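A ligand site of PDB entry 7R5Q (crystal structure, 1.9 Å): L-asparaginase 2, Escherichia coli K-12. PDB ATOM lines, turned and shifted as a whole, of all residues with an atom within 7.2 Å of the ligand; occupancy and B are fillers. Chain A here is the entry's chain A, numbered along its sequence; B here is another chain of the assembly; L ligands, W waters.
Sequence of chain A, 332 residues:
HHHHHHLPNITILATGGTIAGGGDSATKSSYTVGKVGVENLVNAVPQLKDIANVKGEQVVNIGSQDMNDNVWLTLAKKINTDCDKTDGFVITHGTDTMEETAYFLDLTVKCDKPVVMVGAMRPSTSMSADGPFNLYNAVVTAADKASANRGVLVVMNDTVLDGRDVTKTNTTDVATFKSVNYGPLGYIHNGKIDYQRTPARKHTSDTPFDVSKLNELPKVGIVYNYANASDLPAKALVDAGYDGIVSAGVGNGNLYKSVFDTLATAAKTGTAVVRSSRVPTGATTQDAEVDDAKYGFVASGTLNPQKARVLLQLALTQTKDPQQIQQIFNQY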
ATOM      1  N   GLY A  16       4.295 -12.306  22.224  1.00  0.00           N
ATOM      2  CA  GLY A  16       5.348 -13.289  22.010  1.00  0.00           C
ATOM      3  C   GLY A  16       5.181 -14.054  20.710  1.00  0.00           C
ATOM      4  O   GLY A  16       4.509 -13.583  19.788  1.00  0.00           O
ATOM      5  N   GLY A  17       5.800 -15.227  20.597  1.00  0.00           N
ATOM      6  CA  GLY A  17       5.550 -16.079  19.452  1.00  0.00           C
ATOM      7  C   GLY A  17       4.114 -16.567  19.434  1.00  0.00           C
ATOM      8  O   GLY A  17       3.355 -16.394  20.381  1.00  0.00           O
ATOM      9  N   THR A  18       3.732 -17.209  18.336  1.00  0.00           N
ATOM     10  CA  THR A  18       2.411 -17.815  18.285  1.00  0.00           C
ATOM     11  C   THR A  18       2.315 -18.906  19.340  1.00  0.00           C
ATOM     12  O   THR A  18       3.266 -19.637  19.598  1.00  0.00           O
ATOM     13  CB  THR A  18       2.121 -18.392  16.908  1.00  0.00           C
ATOM     14  OG1 THR A  18       2.867 -19.600  16.719  1.00  0.00           O
ATOM     15  CG2 THR A  18       2.503 -17.367  15.829  1.00  0.00           C
ATOM     16  N   ILE A  19       1.151 -19.001  19.991  1.00  0.00           N
ATOM     17  CA  ILE A  19       0.883 -20.140  20.870  1.00  0.00           C
ATOM     18  C   ILE A  19       0.133 -21.227  20.110  1.00  0.00           C
ATOM     19  O   ILE A  19      -0.024 -22.346  20.629  1.00  0.00           O
ATOM     20  CB  ILE A  19       0.121 -19.669  22.119  1.00  0.00           C
ATOM     21  CG1 ILE A  19      -1.329 -19.360  21.790  1.00  0.00           C
ATOM     22  CG2 ILE A  19       0.770 -18.398  22.733  1.00  0.00           C
ATOM     23  CD1 ILE A  19      -2.180 -19.086  22.988  1.00  0.00           C
ATOM     24  N   ILE A  62       8.408 -11.144  22.611  1.00  0.00           N
ATOM     25  CA  ILE A  62       9.424 -11.533  23.581  1.00  0.00           C
ATOM     26  C   ILE A  62       8.965 -12.722  24.386  1.00  0.00           C
ATOM     27  O   ILE A  62       7.766 -13.011  24.486  1.00  0.00           O
ATOM     28  CB  ILE A  62       9.789 -10.375  24.535  1.00  0.00           C
ATOM     29  CG1 ILE A  62       8.545  -9.755  25.183  1.00  0.00           C
ATOM     30  CG2 ILE A  62      10.538  -9.302  23.795  1.00  0.00           C
ATOM     31  CD1 ILE A  62       8.901  -8.931  26.435  1.00  0.00           C
ATOM     32  N   GLY A  63       9.935 -13.435  24.958  1.00  0.00           N
ATOM     33  CA  GLY A  63       9.619 -14.401  25.968  1.00  0.00           C
ATOM     34  C   GLY A  63       9.232 -13.681  27.239  1.00  0.00           C
ATOM     35  O   GLY A  63       9.797 -12.645  27.594  1.00  0.00           O
ATOM     36  N   SER A  64       8.225 -14.204  27.926  1.00  0.00           N
ATOM     37  CA  SER A  64       7.674 -13.444  29.045  1.00  0.00           C
ATOM     38  C   SER A  64       8.616 -13.421  30.244  1.00  0.00           C
ATOM     39  O   SER A  64       8.394 -12.636  31.167  1.00  0.00           O
ATOM     40  CB  SER A  64       6.285 -13.980  29.461  1.00  0.00           C
ATOM     41  OG  SER A  64       6.378 -15.116  30.265  1.00  0.00           O
ATOM     42  N   GLN A  65       9.685 -14.231  30.246  1.00  0.00           N
ATOM     43  CA  GLN A  65      10.680 -14.079  31.298  1.00  0.00           C
ATOM     44  C   GLN A  65      11.405 -12.733  31.203  1.00  0.00           C
ATOM     45  O   GLN A  65      12.066 -12.347  32.163  1.00  0.00           O
ATOM     46  CB  GLN A  65      11.700 -15.195  31.273  1.00  0.00           C
ATOM     47  CG  GLN A  65      12.644 -15.181  30.082  1.00  0.00           C
ATOM     48  CD  GLN A  65      12.065 -15.910  28.877  1.00  0.00           C
ATOM     49  OE1 GLN A  65      10.848 -16.097  28.769  1.00  0.00           O
ATOM     50  NE2 GLN A  65      12.937 -16.309  27.983  1.00  0.00           N
ATOM     51  N   ASP A  66      11.311 -12.060  30.057  1.00  0.00           N
ATOM     52  CA  ASP A  66      11.878 -10.736  29.798  1.00  0.00           C
ATOM     53  C   ASP A  66      10.840  -9.625  29.903  1.00  0.00           C
ATOM     54  O   ASP A  66      11.140  -8.451  29.594  1.00  0.00           O
ATOM     55  CB  ASP A  66      12.513 -10.719  28.406  1.00  0.00           C
ATOM     56  CG  ASP A  66      13.783 -11.597  28.312  1.00  0.00           C
ATOM     57  OD1 ASP A  66      14.352 -11.885  29.388  1.00  0.00           O
ATOM     58  OD2 ASP A  66      14.167 -11.974  27.187  1.00  0.00           O
ATOM     59  N   HIS A  93       0.282 -14.410  25.479  1.00  0.00           N
ATOM     60  CA  HIS A  93       1.384 -14.033  26.374  1.00  0.00           C
ATOM     61  C   HIS A  93       2.176 -15.226  26.901  1.00  0.00           C
ATOM     62  O   HIS A  93       1.551 -16.261  27.145  1.00  0.00           O
ATOM     63  CB  HIS A  93       0.729 -13.362  27.571  1.00  0.00           C
ATOM     64  CG  HIS A  93       1.618 -12.436  28.321  1.00  0.00           C
ATOM     65  ND1 HIS A  93       2.395 -12.842  29.382  1.00  0.00           N
ATOM     66  CD2 HIS A  93       1.813 -11.102  28.204  1.00  0.00           C
ATOM     67  CE1 HIS A  93       3.048 -11.818  29.874  1.00  0.00           C
ATOM     68  NE2 HIS A  93       2.702 -10.733  29.182  1.00  0.00           N
ATOM     69  N   GLY A  94       3.510 -15.122  27.130  1.00  0.00           N
ATOM     70  CA  GLY A  94       4.206 -16.261  27.684  1.00  0.00           C
ATOM     71  C   GLY A  94       3.692 -16.531  29.082  1.00  0.00           C
ATOM     72  O   GLY A  94       3.227 -15.623  29.792  1.00  0.00           O
ATOM     73  N   THR A  95       3.747 -17.803  29.491  1.00  0.00           N
ATOM     74  CA  THR A  95       3.128 -18.138  30.749  1.00  0.00           C
ATOM     75  C   THR A  95       3.941 -17.699  31.955  1.00  0.00           C
ATOM     76  O   THR A  95       3.368 -17.510  33.032  1.00  0.00           O
ATOM     77  CB  THR A  95       2.867 -19.639  30.810  1.00  0.00           C
ATOM     78  OG1 THR A  95       4.120 -20.322  30.721  1.00  0.00           O
ATOM     79  CG2 THR A  95       1.932 -20.103  29.689  1.00  0.00           C
ATOM     80  N   ASP A  96       5.258 -17.526  31.814  1.00  0.00           N
ATOM     81  CA  ASP A  96       6.122 -17.360  33.001  1.00  0.00           C
ATOM     82  C   ASP A  96       5.747 -16.138  33.847  1.00  0.00           C
ATOM     83  O   ASP A  96       5.807 -16.199  35.087  1.00  0.00           O
ATOM     84  CB  ASP A  96       7.588 -17.254  32.608  1.00  0.00           C
ATOM     85  CG  ASP A  96       8.195 -18.573  32.143  1.00  0.00           C
ATOM     86  OD1 ASP A  96       7.499 -19.626  32.196  1.00  0.00           O
ATOM     87  OD2 ASP A  96       9.376 -18.566  31.703  1.00  0.00           O
ATOM     88  N   THR A  97       5.352 -15.021  33.208  1.00  0.00           N
ATOM     89  CA  THR A  97       4.998 -13.819  33.958  1.00  0.00           C
ATOM     90  C   THR A  97       3.595 -13.356  33.618  1.00  0.00           C
ATOM     91  O   THR A  97       3.204 -12.238  33.964  1.00  0.00           O
ATOM     92  CB  THR A  97       6.011 -12.683  33.740  1.00  0.00           C
ATOM     93  OG1 THR A  97       5.996 -12.286  32.374  1.00  0.00           O
ATOM     94  CG2 THR A  97       7.444 -13.123  34.165  1.00  0.00           C
ATOM     95  N   MET A  98       2.814 -14.215  32.998  1.00  0.00           N
ATOM     96  CA  MET A  98       1.466 -13.833  32.685  1.00  0.00           C
ATOM     97  C   MET A  98       0.744 -13.341  33.935  1.00  0.00           C
ATOM     98  O   MET A  98      -0.084 -12.431  33.861  1.00  0.00           O
ATOM     99  CB  MET A  98       0.723 -15.004  32.031  1.00  0.00           C
ATOM    100  CG  MET A  98      -0.682 -14.619  31.594  1.00  0.00           C
ATOM    101  SD  MET A  98      -1.435 -15.642  30.446  1.00  0.00           S
ATOM    102  CE  MET A  98      -0.950 -17.236  30.946  1.00  0.00           C
ATOM    103  N   GLY A 119      -2.044 -18.210  27.137  1.00  0.00           N
ATOM    104  CA  GLY A 119      -0.755 -18.711  26.714  1.00  0.00           C
ATOM    105  C   GLY A 119      -0.827 -20.208  26.502  1.00  0.00           C
ATOM    106  O   GLY A 119      -1.927 -20.788  26.443  1.00  0.00           O
ATOM    107  N   ALA A 120       0.330 -20.825  26.330  1.00  0.00           N
ATOM    108  CA  ALA A 120       0.415 -22.259  26.111  1.00  0.00           C
ATOM    109  C   ALA A 120       1.586 -22.803  26.900  1.00  0.00           C
ATOM    110  O   ALA A 120       2.670 -22.234  26.882  1.00  0.00           O
ATOM    111  CB  ALA A 120       0.576 -22.569  24.614  1.00  0.00           C
ATOM    112  N   MET A 121       1.378 -23.964  27.532  1.00  0.00           N
ATOM    113  CA  MET A 121       2.430 -24.624  28.298  1.00  0.00           C
ATOM    114  C   MET A 121       3.224 -25.616  27.455  1.00  0.00           C
ATOM    115  O   MET A 121       4.331 -25.992  27.852  1.00  0.00           O
ATOM    116  CB  MET A 121       1.818 -25.312  29.510  1.00  0.00           C
ATOM    117  CG  MET A 121       1.372 -24.343  30.567  1.00  0.00           C
ATOM    118  SD  MET A 121       2.808 -23.551  31.314  1.00  0.00           S
ATOM    119  CE  MET A 121       3.516 -24.830  32.320  1.00  0.00           C
ATOM    120  N   ARG A 122       2.701 -26.003  26.309  1.00  0.00           N
ATOM    121  CA  ARG A 122       3.411 -26.833  25.344  1.00  0.00           C
ATOM    122  C   ARG A 122       3.722 -26.050  24.067  1.00  0.00           C
ATOM    123  O   ARG A 122       2.949 -25.164  23.666  1.00  0.00           O
ATOM    124  CB  ARG A 122       2.571 -28.070  25.001  1.00  0.00           C
ATOM    125  CG  ARG A 122       2.409 -28.959  26.219  1.00  0.00           C
ATOM    126  CD  ARG A 122       1.415 -30.107  25.940  1.00  0.00           C
ATOM    127  NE  ARG A 122       1.251 -30.966  27.098  1.00  0.00           N
ATOM    128  CZ  ARG A 122       0.231 -31.806  27.236  1.00  0.00           C
ATOM    129  NH1 ARG A 122      -0.709 -31.910  26.309  1.00  0.00           N
ATOM    130  NH2 ARG A 122       0.141 -32.545  28.342  1.00  0.00           N
ATOM    131  N   MET A 156      -7.096 -20.399  30.743  1.00  0.00           N
ATOM    132  CA  MET A 156      -6.141 -21.479  30.608  1.00  0.00           C
ATOM    133  C   MET A 156      -6.831 -22.747  31.071  1.00  0.00           C
ATOM    134  O   MET A 156      -7.572 -22.737  32.055  1.00  0.00           O
ATOM    135  CB  MET A 156      -4.882 -21.265  31.445  1.00  0.00           C
ATOM    136  CG  MET A 156      -4.030 -20.129  30.943  1.00  0.00           C
ATOM    137  SD  MET A 156      -3.327 -20.439  29.304  1.00  0.00           S
ATOM    138  CE  MET A 156      -1.916 -21.428  29.771  1.00  0.00           C
ATOM    139  N   LYS A 168       0.829 -19.157  38.435  1.00  0.00           N
ATOM    140  CA  LYS A 168       1.405 -20.350  37.841  1.00  0.00           C
ATOM    141  C   LYS A 168       1.867 -21.243  38.963  1.00  0.00           C
ATOM    142  O   LYS A 168       2.817 -20.912  39.669  1.00  0.00           O
ATOM    143  CB  LYS A 168       2.547 -19.968  36.912  1.00  0.00           C
ATOM    144  CG  LYS A 168       3.167 -21.083  36.232  1.00  0.00           C
ATOM    145  CD  LYS A 168       3.938 -20.567  34.993  1.00  0.00           C
ATOM    146  CE  LYS A 168       4.588 -21.678  34.261  1.00  0.00           C
ATOM    147  NZ  LYS A 168       5.238 -21.198  33.005  1.00  0.00           N
ATOM    148  N   PHE A 177      -2.176 -23.009  35.808  1.00  0.00           N
ATOM    149  CA  PHE A 177      -2.797 -21.764  36.284  1.00  0.00           C
ATOM    150  C   PHE A 177      -4.012 -22.017  37.166  1.00  0.00           C
ATOM    151  O   PHE A 177      -5.000 -22.593  36.722  1.00  0.00           O
ATOM    152  CB  PHE A 177      -3.144 -20.806  35.126  1.00  0.00           C
ATOM    153  CG  PHE A 177      -1.932 -20.164  34.557  1.00  0.00           C
ATOM    154  CD1 PHE A 177      -1.312 -19.112  35.174  1.00  0.00           C
ATOM    155  CD2 PHE A 177      -1.362 -20.702  33.420  1.00  0.00           C
ATOM    156  CE1 PHE A 177      -0.153 -18.573  34.646  1.00  0.00           C
ATOM    157  CE2 PHE A 177      -0.229 -20.209  32.904  1.00  0.00           C
ATOM    158  CZ  PHE A 177       0.399 -19.139  33.506  1.00  0.00           C
ATOM    159  N   VAL B 250      11.466 -17.919  36.889  1.00  0.00           N
ATOM    160  CA  VAL B 250      10.077 -17.897  36.475  1.00  0.00           C
ATOM    161  C   VAL B 250       9.793 -19.129  35.639  1.00  0.00           C
ATOM    162  O   VAL B 250      10.661 -19.605  34.882  1.00  0.00           O
ATOM    163  CB  VAL B 250       9.733 -16.598  35.711  1.00  0.00           C
ATOM    164  CG1 VAL B 250       9.893 -15.416  36.647  1.00  0.00           C
ATOM    165  CG2 VAL B 250      10.563 -16.406  34.512  1.00  0.00           C
ATOM    166  N   GLY B 251       8.584 -19.657  35.768  1.00  0.00           N
ATOM    167  CA  GLY B 251       8.263 -20.822  34.988  1.00  0.00           C
ATOM    168  C   GLY B 251       9.240 -21.964  35.228  1.00  0.00           C
ATOM    169  O   GLY B 251       9.613 -22.280  36.345  1.00  0.00           O
ATOM    170  N   ASN B 252       9.659 -22.607  34.146  1.00  0.00           N
ATOM    171  CA  ASN B 252      10.613 -23.709  34.252  1.00  0.00           C
ATOM    172  C   ASN B 252      12.040 -23.172  34.400  1.00  0.00           C
ATOM    173  O   ASN B 252      12.912 -23.409  33.555  1.00  0.00           O
ATOM    174  CB  ASN B 252      10.509 -24.605  33.038  1.00  0.00           C
ATOM    175  CG  ASN B 252      11.170 -25.961  33.257  1.00  0.00           C
ATOM    176  OD1 ASN B 252      11.961 -26.149  34.197  1.00  0.00           O
ATOM    177  ND2 ASN B 252      10.817 -26.915  32.390  1.00  0.00           N
ATOM    178  N   ASN B 254      13.390 -20.160  34.308  1.00  0.00           N
ATOM    179  CA  ASN B 254      13.859 -19.103  33.420  1.00  0.00           C
ATOM    180  C   ASN B 254      14.246 -17.835  34.186  1.00  0.00           C
ATOM    181  O   ASN B 254      13.864 -17.609  35.333  1.00  0.00           O
ATOM    182  CB  ASN B 254      12.794 -18.777  32.382  1.00  0.00           C
ATOM    183  CG  ASN B 254      12.596 -19.904  31.407  1.00  0.00           C
ATOM    184  OD1 ASN B 254      13.576 -20.379  30.844  1.00  0.00           O
ATOM    185  ND2 ASN B 254      11.348 -20.420  31.276  1.00  0.00           N
ATOM    186  N   GLU B 289      14.321 -24.578  28.251  1.00  0.00           N
ATOM    187  CA  GLU B 289      14.622 -23.334  27.567  1.00  0.00           C
ATOM    188  C   GLU B 289      16.068 -22.897  27.734  1.00  0.00           C
ATOM    189  O   GLU B 289      16.565 -22.168  26.871  1.00  0.00           O
ATOM    190  CB  GLU B 289      13.698 -22.206  28.073  1.00  0.00           C
ATOM    191  CG  GLU B 289      12.951 -21.521  26.967  1.00  0.00           C
ATOM    192  CD  GLU B 289      11.830 -20.646  27.483  1.00  0.00           C
ATOM    193  OE1 GLU B 289      10.914 -21.188  28.150  1.00  0.00           O
ATOM    194  OE2 GLU B 289      11.886 -19.420  27.223  1.00  0.00           O
HETATM  195  N1  LIG L   1       9.694 -18.700  28.863  1.00  0.00           N
HETATM  196  C1  LIG L   1       8.517 -18.797  27.990  1.00  0.00           C
HETATM  197  C2  LIG L   1       7.641 -17.579  28.180  1.00  0.00           C
HETATM  198  O1  LIG L   1       7.152 -17.392  29.315  1.00  0.00           O
HETATM  199  C3  LIG L   1       7.697 -20.051  28.287  1.00  0.00           C
HETATM  200  C4  LIG L   1       6.753 -20.435  27.137  1.00  0.00           C
HETATM  201  C5  LIG L   1       5.411 -19.718  27.151  1.00  0.00           C
HETATM  202  O2  LIG L   1       4.758 -19.677  28.214  1.00  0.00           O
HETATM  203  O3  LIG L   1       4.979 -19.224  26.083  1.00  0.00           O
HETATM  204  O4  LIG L   1       7.418 -16.772  27.276  1.00  0.00           O
HETATM  205  O   HOH W   1       2.408 -18.754  26.003  1.00  0.00           O
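The backbone NH of Thr 95 sits at hydrogen-bond distance from an oxygen (O2) of the ligand. An oxygen (O2) of the ligand is in hydrogen-bond range of the side-chain hydroxyl (OG1) of Thr 95 (2.7 Å). The backbone NH of Ser 64 sits at hydrogen-bond distance from an oxygen (O4) of the ligand (2.8 Å). OG of Ser 64 lies within hydrogen-bond range of O1 of the ligand (2.6 Å). OE2 of Glu 289 of chain B lies within salt-bridge range of N1 of the ligand. The side-chain amide oxygen (OE1) of Gln 65 lies within hydrogen-bond range of a nitrogen (N1) of the ligand, 2.8 Å away. The backbone NH (N) of Asp 96 sits at hydrogen-bond distance from an oxygen (O1) of the ligand (3.1 Å). The side-chain carboxylate (OD2) of Asp 96 lies within salt-bridge range of a nitrogen (N1) of the ligand (2.9 Å). ND2 of Asn 254 of chain B sits close to N1 of the ligand (3.4 Å).
OG1 of Thr 95 lies within hydrogen-bond range of SD of Met 121, 3.5 Å away. N of Asp 96 lies within hydrogen-bond range of OG of Ser 64 (3.1 Å). The side-chain hydroxyl (OG) of Ser 64 is in hydrogen-bond range of the backbone carbonyl oxygen (O) of Gly 94 (3.2 Å). O of Ser 64 is in hydrogen-bond range of OG1 of Thr 97 (2.7 Å). OE2 of Glu 289 of chain B is in hydrogen-bond range of NE2 of Gln 65. The side-chain carboxylate of Glu 289 of chain B sits at hydrogen-bond distance from the side-chain amide nitrogen of Asn 254 of chain B. The side-chain carboxylate (OD2) of Asp 96 is in hydrogen-bond range of the side-chain amide nitrogen (ND2) of Asn 254 of chain B, 2.7 Å away. The side-chain carboxylate of Asp 96 is in salt-bridge range of the side-chain amino group of Lys 168, 2.9 Å away.
Residues that only touch the ligand: Gly 63 (3.5 Å), Gly 94 (3.3 Å) and Ala 120 (3.6 Å). Within 4 Å of the ligand: Gly 63, Ser 64, Gln 65, Gly 94, Thr 95, Asp 96, Ala 120, Asn 254 of chain B and Glu 289 of chain B. Along chain A the residues within 4 Å of the ligand span positions 63 to 120.
Water W1 lies within hydrogen-bond range of O3 of the ligand (2.6 Å), O of His 93 (2.9 Å) and N of Ala 120 (3.0 Å).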
